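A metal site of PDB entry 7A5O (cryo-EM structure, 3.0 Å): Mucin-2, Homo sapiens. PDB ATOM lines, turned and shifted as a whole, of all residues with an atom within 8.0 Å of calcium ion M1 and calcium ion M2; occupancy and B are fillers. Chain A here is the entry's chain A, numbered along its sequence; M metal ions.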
ATOM      1  N   ILE A1289       0.045 -22.290 -12.635  1.00  0.00           N
ATOM      2  CA  ILE A1289       0.973 -22.573 -13.725  1.00  0.00           C
ATOM      3  C   ILE A1289       1.629 -23.912 -13.430  1.00  0.00           C
ATOM      4  O   ILE A1289       2.476 -24.011 -12.530  1.00  0.00           O
ATOM      5  CB  ILE A1289       2.034 -21.463 -13.877  1.00  0.00           C
ATOM      6  CG1 ILE A1289       1.350 -20.140 -14.201  1.00  0.00           C
ATOM      7  CG2 ILE A1289       3.007 -21.815 -14.974  1.00  0.00           C
ATOM      8  CD1 ILE A1289       2.270 -18.946 -14.102  1.00  0.00           C
ATOM      9  N   ASN A1290       1.238 -24.937 -14.179  1.00  0.00           N
ATOM     10  CA  ASN A1290       1.860 -26.259 -14.112  1.00  0.00           C
ATOM     11  C   ASN A1290       2.452 -26.517 -15.493  1.00  0.00           C
ATOM     12  O   ASN A1290       1.825 -27.133 -16.349  1.00  0.00           O
ATOM     13  CB  ASN A1290       0.854 -27.339 -13.725  1.00  0.00           C
ATOM     14  CG  ASN A1290       1.512 -28.646 -13.352  1.00  0.00           C
ATOM     15  OD1 ASN A1290       2.735 -28.751 -13.270  1.00  0.00           O
ATOM     16  ND2 ASN A1290       0.703 -29.680 -13.181  1.00  0.00           N
ATOM     17  N   GLU A1291       3.674 -26.035 -15.706  1.00  0.00           N
ATOM     18  CA  GLU A1291       4.320 -26.127 -17.005  1.00  0.00           C
ATOM     19  C   GLU A1291       5.527 -27.053 -16.994  1.00  0.00           C
ATOM     20  O   GLU A1291       6.368 -26.991 -17.900  1.00  0.00           O
ATOM     21  CB  GLU A1291       4.727 -24.737 -17.497  1.00  0.00           C
ATOM     22  N   ASP A1292       5.635 -27.912 -15.979  1.00  0.00           N
ATOM     23  CA  ASP A1292       6.764 -28.825 -15.866  1.00  0.00           C
ATOM     24  C   ASP A1292       6.302 -30.026 -15.053  1.00  0.00           C
ATOM     25  O   ASP A1292       5.307 -29.964 -14.338  1.00  0.00           O
ATOM     26  CB  ASP A1292       7.964 -28.113 -15.218  1.00  0.00           C
ATOM     27  CG  ASP A1292       9.260 -28.868 -15.384  1.00  0.00           C
ATOM     28  OD1 ASP A1292       9.261 -29.961 -15.991  1.00  0.00           O
ATOM     29  OD2 ASP A1292      10.304 -28.365 -14.916  1.00  0.00           O
ATOM     30  N   HIS A1293       7.031 -31.128 -15.188  1.00  0.00           N
ATOM     31  CA  HIS A1293       6.657 -32.381 -14.549  1.00  0.00           C
ATOM     32  C   HIS A1293       7.916 -33.091 -14.070  1.00  0.00           C
ATOM     33  O   HIS A1293       9.011 -32.854 -14.598  1.00  0.00           O
ATOM     34  CB  HIS A1293       5.877 -33.286 -15.513  1.00  0.00           C
ATOM     35  CG  HIS A1293       4.551 -32.730 -15.908  1.00  0.00           C
ATOM     36  ND1 HIS A1293       3.464 -32.760 -15.065  1.00  0.00           N
ATOM     37  CD2 HIS A1293       4.151 -32.087 -17.031  1.00  0.00           C
ATOM     38  CE1 HIS A1293       2.434 -32.180 -15.666  1.00  0.00           C
ATOM     39  NE2 HIS A1293       2.826 -31.766 -16.854  1.00  0.00           N
ATOM     40  N   PRO A1294       7.796 -33.947 -13.056  1.00  0.00           N
ATOM     41  CA  PRO A1294       8.971 -34.752 -12.655  1.00  0.00           C
ATOM     42  C   PRO A1294       9.280 -35.880 -13.627  1.00  0.00           C
ATOM     43  O   PRO A1294      10.454 -36.189 -13.843  1.00  0.00           O
ATOM     44  CB  PRO A1294       8.559 -35.288 -11.276  1.00  0.00           C
ATOM     45  CG  PRO A1294       7.532 -34.338 -10.798  1.00  0.00           C
ATOM     46  CD  PRO A1294       6.768 -33.934 -12.009  1.00  0.00           C
ATOM     47  N   SER A1295       8.263 -36.506 -14.204  1.00  0.00           N
ATOM     48  CA  SER A1295       8.450 -37.612 -15.133  1.00  0.00           C
ATOM     49  C   SER A1295       8.547 -37.155 -16.587  1.00  0.00           C
ATOM     50  O   SER A1295       8.262 -37.937 -17.496  1.00  0.00           O
ATOM     51  CB  SER A1295       7.304 -38.625 -14.983  1.00  0.00           C
ATOM     52  OG  SER A1295       7.443 -39.698 -15.894  1.00  0.00           O
ATOM     53  N   SER A1296       8.924 -35.895 -16.808  1.00  0.00           N
ATOM     54  CA  SER A1296       9.160 -35.359 -18.143  1.00  0.00           C
ATOM     55  C   SER A1296      10.102 -34.172 -17.999  1.00  0.00           C
ATOM     56  O   SER A1296      10.533 -33.826 -16.900  1.00  0.00           O
ATOM     57  CB  SER A1296       7.852 -34.945 -18.839  1.00  0.00           C
ATOM     58  OG  SER A1296       7.040 -36.070 -19.102  1.00  0.00           O
ATOM     59  N   GLY A1297      10.433 -33.545 -19.125  1.00  0.00           N
ATOM     60  CA  GLY A1297      11.378 -32.460 -19.129  1.00  0.00           C
ATOM     61  C   GLY A1297      12.819 -32.952 -19.082  1.00  0.00           C
ATOM     62  O   GLY A1297      13.108 -34.146 -19.238  1.00  0.00           O
ATOM     63  N   SER A1298      13.728 -32.004 -18.861  1.00  0.00           N
ATOM     64  CA  SER A1298      15.142 -32.342 -18.785  1.00  0.00           C
ATOM     65  C   SER A1298      15.883 -31.553 -17.711  1.00  0.00           C
ATOM     66  O   SER A1298      17.133 -31.573 -17.701  1.00  0.00           O
ATOM     67  CB  SER A1298      15.820 -32.134 -20.141  1.00  0.00           C
ATOM     68  OG  SER A1298      15.283 -33.015 -21.110  1.00  0.00           O
ATOM     69  N   ASP A1299      15.196 -30.862 -16.810  1.00  0.00           N
ATOM     70  CA  ASP A1299      15.840 -30.101 -15.754  1.00  0.00           C
ATOM     71  C   ASP A1299      16.044 -30.898 -14.473  1.00  0.00           C
ATOM     72  O   ASP A1299      16.422 -30.301 -13.450  1.00  0.00           O
ATOM     73  CB  ASP A1299      15.043 -28.811 -15.472  1.00  0.00           C
ATOM     74  CG  ASP A1299      13.588 -29.075 -15.107  1.00  0.00           C
ATOM     75  OD1 ASP A1299      13.148 -30.236 -15.143  1.00  0.00           O
ATOM     76  OD2 ASP A1299      12.889 -28.094 -14.766  1.00  0.00           O
ATOM     77  N   ASP A1300      15.793 -32.218 -14.511  1.00  0.00           N
ATOM     78  CA  ASP A1300      16.067 -33.175 -13.425  1.00  0.00           C
ATOM     79  C   ASP A1300      15.286 -32.811 -12.161  1.00  0.00           C
ATOM     80  O   ASP A1300      15.823 -32.801 -11.049  1.00  0.00           O
ATOM     81  CB  ASP A1300      17.579 -33.277 -13.160  1.00  0.00           C
ATOM     82  CG  ASP A1300      17.968 -34.518 -12.371  1.00  0.00           C
ATOM     83  OD1 ASP A1300      17.076 -35.330 -12.048  1.00  0.00           O
ATOM     84  OD2 ASP A1300      19.163 -34.678 -12.073  1.00  0.00           O
ATOM     85  N   GLY A1301      14.006 -32.501 -12.320  1.00  0.00           N
ATOM     86  CA  GLY A1301      13.198 -32.073 -11.193  1.00  0.00           C
ATOM     87  C   GLY A1301      11.924 -31.368 -11.601  1.00  0.00           C
ATOM     88  O   GLY A1301      11.202 -31.854 -12.468  1.00  0.00           O
ATOM     89  N   ASP A1302      11.645 -30.225 -10.995  1.00  0.00           N
ATOM     90  CA  ASP A1302      10.436 -29.475 -11.301  1.00  0.00           C
ATOM     91  C   ASP A1302      10.710 -28.002 -11.041  1.00  0.00           C
ATOM     92  O   ASP A1302      11.056 -27.621  -9.921  1.00  0.00           O
ATOM     93  CB  ASP A1302       9.255 -29.967 -10.456  1.00  0.00           C
ATOM     94  CG  ASP A1302       7.919 -29.471 -10.957  1.00  0.00           C
ATOM     95  OD1 ASP A1302       7.881 -28.737 -11.962  1.00  0.00           O
ATOM     96  OD2 ASP A1302       6.904 -29.820 -10.351  1.00  0.00           O
ATOM     97  N   ARG A1303      10.580 -27.175 -12.080  1.00  0.00           N
ATOM     98  CA  ARG A1303      10.850 -25.751 -11.970  1.00  0.00           C
ATOM     99  C   ARG A1303       9.762 -24.974 -12.684  1.00  0.00           C
ATOM    100  O   ARG A1303       9.472 -25.231 -13.850  1.00  0.00           O
ATOM    101  CB  ARG A1303      12.224 -25.400 -12.566  1.00  0.00           C
ATOM    102  CG  ARG A1303      13.395 -25.922 -11.753  1.00  0.00           C
ATOM    103  CD  ARG A1303      14.736 -25.585 -12.364  1.00  0.00           C
ATOM    104  NE  ARG A1303      15.824 -26.132 -11.572  1.00  0.00           N
ATOM    105  CZ  ARG A1303      17.112 -26.034 -11.895  1.00  0.00           C
ATOM    106  NH1 ARG A1303      17.471 -25.405 -12.998  1.00  0.00           N
ATOM    107  NH2 ARG A1303      18.037 -26.563 -11.103  1.00  0.00           N
ATOM    108  N   GLU A1304       9.160 -24.024 -11.974  1.00  0.00           N
ATOM    109  CA  GLU A1304       8.036 -23.238 -12.469  1.00  0.00           C
ATOM    110  C   GLU A1304       8.388 -21.762 -12.350  1.00  0.00           C
ATOM    111  O   GLU A1304       8.593 -21.255 -11.246  1.00  0.00           O
ATOM    112  CB  GLU A1304       6.760 -23.547 -11.694  1.00  0.00           C
ATOM    113  CG  GLU A1304       6.232 -24.953 -11.891  1.00  0.00           C
ATOM    114  CD  GLU A1304       5.714 -25.180 -13.286  1.00  0.00           C
ATOM    115  OE1 GLU A1304       5.177 -24.226 -13.892  1.00  0.00           O
ATOM    116  OE2 GLU A1304       5.844 -26.310 -13.797  1.00  0.00           O
ATOM    117  N   ARG A1319       2.181 -24.627  -4.138  1.00  0.00           N
ATOM    118  CA  ARG A1319       1.340 -25.761  -3.775  1.00  0.00           C
ATOM    119  C   ARG A1319       1.578 -26.942  -4.693  1.00  0.00           C
ATOM    120  O   ARG A1319       2.356 -26.868  -5.650  1.00  0.00           O
ATOM    121  CB  ARG A1319      -0.154 -25.382  -3.784  1.00  0.00           C
ATOM    122  CG  ARG A1319      -0.514 -24.358  -2.738  1.00  0.00           C
ATOM    123  CD  ARG A1319      -0.342 -24.977  -1.374  1.00  0.00           C
ATOM    124  NE  ARG A1319      -0.617 -24.040  -0.289  1.00  0.00           N
ATOM    125  CZ  ARG A1319      -1.808 -23.852   0.252  1.00  0.00           C
ATOM    126  NH1 ARG A1319      -2.854 -24.526  -0.206  1.00  0.00           N
ATOM    127  NH2 ARG A1319      -1.961 -22.983   1.234  1.00  0.00           N
ATOM    128  N   SER A1320       0.922 -28.057  -4.383  1.00  0.00           N
ATOM    129  CA  SER A1320       1.050 -29.293  -5.132  1.00  0.00           C
ATOM    130  C   SER A1320      -0.200 -29.550  -5.966  1.00  0.00           C
ATOM    131  O   SER A1320      -1.269 -29.026  -5.683  1.00  0.00           O
ATOM    132  CB  SER A1320       1.292 -30.487  -4.214  1.00  0.00           C
ATOM    133  OG  SER A1320       1.393 -31.692  -4.953  1.00  0.00           O
ATOM    134  N   VAL A1321      -0.036 -30.388  -6.986  1.00  0.00           N
ATOM    135  CA  VAL A1321      -1.121 -30.620  -7.931  1.00  0.00           C
ATOM    136  C   VAL A1321      -2.157 -31.568  -7.341  1.00  0.00           C
ATOM    137  O   VAL A1321      -3.339 -31.246  -7.263  1.00  0.00           O
ATOM    138  CB  VAL A1321      -0.555 -31.146  -9.257  1.00  0.00           C
ATOM    139  CG1 VAL A1321      -1.679 -31.512 -10.187  1.00  0.00           C
ATOM    140  CG2 VAL A1321       0.319 -30.118  -9.870  1.00  0.00           C
ATOM    141  N   PHE A1343      10.326 -21.285  -8.683  1.00  0.00           N
ATOM    142  CA  PHE A1343      10.295 -22.543  -7.942  1.00  0.00           C
ATOM    143  C   PHE A1343      11.393 -23.454  -8.457  1.00  0.00           C
ATOM    144  O   PHE A1343      11.609 -23.541  -9.669  1.00  0.00           O
ATOM    145  CB  PHE A1343       8.930 -23.221  -8.078  1.00  0.00           C
ATOM    146  CG  PHE A1343       8.818 -24.508  -7.326  1.00  0.00           C
ATOM    147  CD1 PHE A1343       8.688 -24.518  -5.955  1.00  0.00           C
ATOM    148  CD2 PHE A1343       8.851 -25.717  -7.996  1.00  0.00           C
ATOM    149  CE1 PHE A1343       8.600 -25.695  -5.265  1.00  0.00           C
ATOM    150  CE2 PHE A1343       8.757 -26.902  -7.306  1.00  0.00           C
ATOM    151  CZ  PHE A1343       8.641 -26.885  -5.943  1.00  0.00           C
ATOM    152  N   CYS A1345      12.896 -27.459  -7.705  1.00  0.00           N
ATOM    153  CA  CYS A1345      13.028 -28.765  -7.064  1.00  0.00           C
ATOM    154  C   CYS A1345      14.043 -29.561  -7.867  1.00  0.00           C
ATOM    155  O   CYS A1345      13.969 -29.599  -9.098  1.00  0.00           O
ATOM    156  CB  CYS A1345      11.680 -29.506  -6.992  1.00  0.00           C
ATOM    157  SG  CYS A1345      11.667 -31.072  -6.058  1.00  0.00           S
ATOM    158  N   ASN A1347      15.938 -33.367  -8.219  1.00  0.00           N
ATOM    159  CA  ASN A1347      15.791 -34.777  -7.833  1.00  0.00           C
ATOM    160  C   ASN A1347      16.978 -35.284  -7.032  1.00  0.00           C
ATOM    161  O   ASN A1347      16.835 -36.254  -6.285  1.00  0.00           O
ATOM    162  CB  ASN A1347      15.613 -35.676  -9.058  1.00  0.00           C
ATOM    163  CG  ASN A1347      14.242 -35.566  -9.676  1.00  0.00           C
ATOM    164  OD1 ASN A1347      13.249 -35.469  -8.973  1.00  0.00           O
ATOM    165  ND2 ASN A1347      14.188 -35.612 -10.997  1.00  0.00           N
ATOM    166  N   TYR A1360       7.698 -34.117  -6.273  1.00  0.00           N
ATOM    167  CA  TYR A1360       6.257 -34.170  -6.471  1.00  0.00           C
ATOM    168  C   TYR A1360       5.903 -33.179  -7.571  1.00  0.00           C
ATOM    169  O   TYR A1360       6.750 -32.457  -8.088  1.00  0.00           O
ATOM    170  CB  TYR A1360       5.539 -33.879  -5.155  1.00  0.00           C
ATOM    171  CG  TYR A1360       5.769 -34.915  -4.078  1.00  0.00           C
ATOM    172  CD1 TYR A1360       6.142 -36.220  -4.394  1.00  0.00           C
ATOM    173  CD2 TYR A1360       5.712 -34.569  -2.738  1.00  0.00           C
ATOM    174  CE1 TYR A1360       6.385 -37.136  -3.405  1.00  0.00           C
ATOM    175  CE2 TYR A1360       5.962 -35.490  -1.753  1.00  0.00           C
ATOM    176  CZ  TYR A1360       6.300 -36.768  -2.091  1.00  0.00           C
ATOM    177  OH  TYR A1360       6.555 -37.704  -1.125  1.00  0.00           O
ATOM    178  N   ASP A1361       4.635 -33.134  -7.948  1.00  0.00           N
ATOM    179  CA  ASP A1361       4.187 -32.274  -9.035  1.00  0.00           C
ATOM    180  C   ASP A1361       3.623 -31.000  -8.421  1.00  0.00           C
ATOM    181  O   ASP A1361       2.649 -31.055  -7.675  1.00  0.00           O
ATOM    182  CB  ASP A1361       3.156 -32.994  -9.885  1.00  0.00           C
ATOM    183  CG  ASP A1361       2.890 -32.299 -11.198  1.00  0.00           C
ATOM    184  OD1 ASP A1361       3.496 -31.248 -11.477  1.00  0.00           O
ATOM    185  OD2 ASP A1361       2.071 -32.831 -11.976  1.00  0.00           O
ATOM    186  N   TYR A1362       4.248 -29.876  -8.728  1.00  0.00           N
ATOM    187  CA  TYR A1362       3.944 -28.592  -8.098  1.00  0.00           C
ATOM    188  C   TYR A1362       3.341 -27.626  -9.112  1.00  0.00           C
ATOM    189  O   TYR A1362       3.390 -27.839 -10.325  1.00  0.00           O
ATOM    190  CB  TYR A1362       5.212 -28.000  -7.494  1.00  0.00           C
ATOM    191  CG  TYR A1362       5.748 -28.722  -6.282  1.00  0.00           C
ATOM    192  CD1 TYR A1362       5.290 -28.430  -5.008  1.00  0.00           C
ATOM    193  CD2 TYR A1362       6.716 -29.713  -6.414  1.00  0.00           C
ATOM    194  CE1 TYR A1362       5.781 -29.075  -3.910  1.00  0.00           C
ATOM    195  CE2 TYR A1362       7.212 -30.375  -5.312  1.00  0.00           C
ATOM    196  CZ  TYR A1362       6.745 -30.049  -4.069  1.00  0.00           C
ATOM    197  OH  TYR A1362       7.230 -30.703  -2.972  1.00  0.00           O
ATOM    198  N   LYS A1363       2.767 -26.549  -8.584  1.00  0.00           N
ATOM    199  CA  LYS A1363       2.141 -25.495  -9.380  1.00  0.00           C
ATOM    200  C   LYS A1363       2.171 -24.215  -8.575  1.00  0.00           C
ATOM    201  O   LYS A1363       2.239 -24.247  -7.343  1.00  0.00           O
ATOM    202  CB  LYS A1363       0.720 -25.880  -9.776  1.00  0.00           C
ATOM    203  CG  LYS A1363      -0.228 -26.018  -8.608  1.00  0.00           C
ATOM    204  CD  LYS A1363      -1.607 -26.444  -9.046  1.00  0.00           C
ATOM    205  CE  LYS A1363      -2.529 -26.553  -7.867  1.00  0.00           C
ATOM    206  NZ  LYS A1363      -3.889 -26.968  -8.286  1.00  0.00           N
ATOM    207  N   ILE A1364       2.161 -23.067  -9.260  1.00  0.00           N
ATOM    208  CA  ILE A1364       2.331 -21.767  -8.603  1.00  0.00           C
ATOM    209  C   ILE A1364       1.352 -20.725  -9.122  1.00  0.00           C
ATOM    210  O   ILE A1364       0.848 -20.795 -10.245  1.00  0.00           O
ATOM    211  CB  ILE A1364       3.773 -21.201  -8.748  1.00  0.00           C
ATOM    212  CG1 ILE A1364       4.131 -21.001 -10.221  1.00  0.00           C
ATOM    213  CG2 ILE A1364       4.797 -22.044  -7.999  1.00  0.00           C
ATOM    214  CD1 ILE A1364       5.403 -20.211 -10.427  1.00  0.00           C
HETATM  215 CA    CA M   1       4.944 -28.986 -12.004  1.00  0.00          CA
HETATM  216 CA    CA M   2      11.125 -31.686 -15.637  1.00  0.00          CA
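Glu 1304 touches calcium ion M1 (OE2 to CA, 3.3 Å).
Within 4 Å of calcium ion M1: Asn 1290, Asp 1292, Asp 1302, Glu 1304, Asp 1361 and Tyr 1362.
The nearest printed residue that does not touch calcium ion M1 is His 1293 (4.4 Å).
Gly 1297 touches calcium ion M2.
Gly 1301 touches calcium ion M2 (O to CA, 3.2 Å).
Six residues have an atom within 4 Å of calcium ion M2: Asp 1292, His 1293, Ser 1296, Gly 1297, Asp 1299 and Gly 1301.
The nearest printed residue that does not touch calcium ion M2 is Ser 1298 (4.2 Å).
The backbone NH of Asp 1292 sits at hydrogen-bond distance from the side-chain carboxylate of Glu 1304, 2.7 Å away.
The side-chain carboxylate (OD2) of Asp 1292 sits at hydrogen-bond distance from the backbone NH (N) of Arg 1303 (3.1 Å).
A ring nitrogen (ND1) of His 1293 sits at hydrogen-bond distance from the side-chain carboxylate (OD2) of Asp 1361, 3.4 Å away.
The backbone carbonyl oxygen of Asp 1302 sits at hydrogen-bond distance from the backbone NH of Cys 1345 (2.9 Å).
O of Asp 1361 is in hydrogen-bond range of N of Val 1321, at 2.9 Å.
ND2 of Asn 1347 lies close to N of Gly 1301, 3.4 Å away.
The side-chain carboxylate (OE2) of Glu 1304 is in hydrogen-bond range of the backbone NH (N) of Glu 1291, at 2.9 Å.
O of Glu 1304 is in hydrogen-bond range of N of Phe 1343.
O of Asp 1292 is bound to calcium ion M1 (2.6 Å).
Calcium ion M1 is bound by OD1 of Asn 1290.
O of Tyr 1362 is bound to calcium ion M1.
OD2 of Asp 1302 is bound to calcium ion M1, 2.7 Å away.
OD1 of Asp 1361 binds calcium ion M1.
Calcium ion M1 has five donor atoms within binding distance.
Slightly farther from calcium ion M1 lies OD1 of Asp 1302 (2.9 Å).
Calcium ion M2 is bound by the side-chain carboxylate of Asp 1299, the backbone carbonyl oxygen of Ser 1296, the side-chain carboxylate of Asp 1292 and the backbone carbonyl oxygen of His 1293.
Calcium ion M2 has four donor atoms within binding distance.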
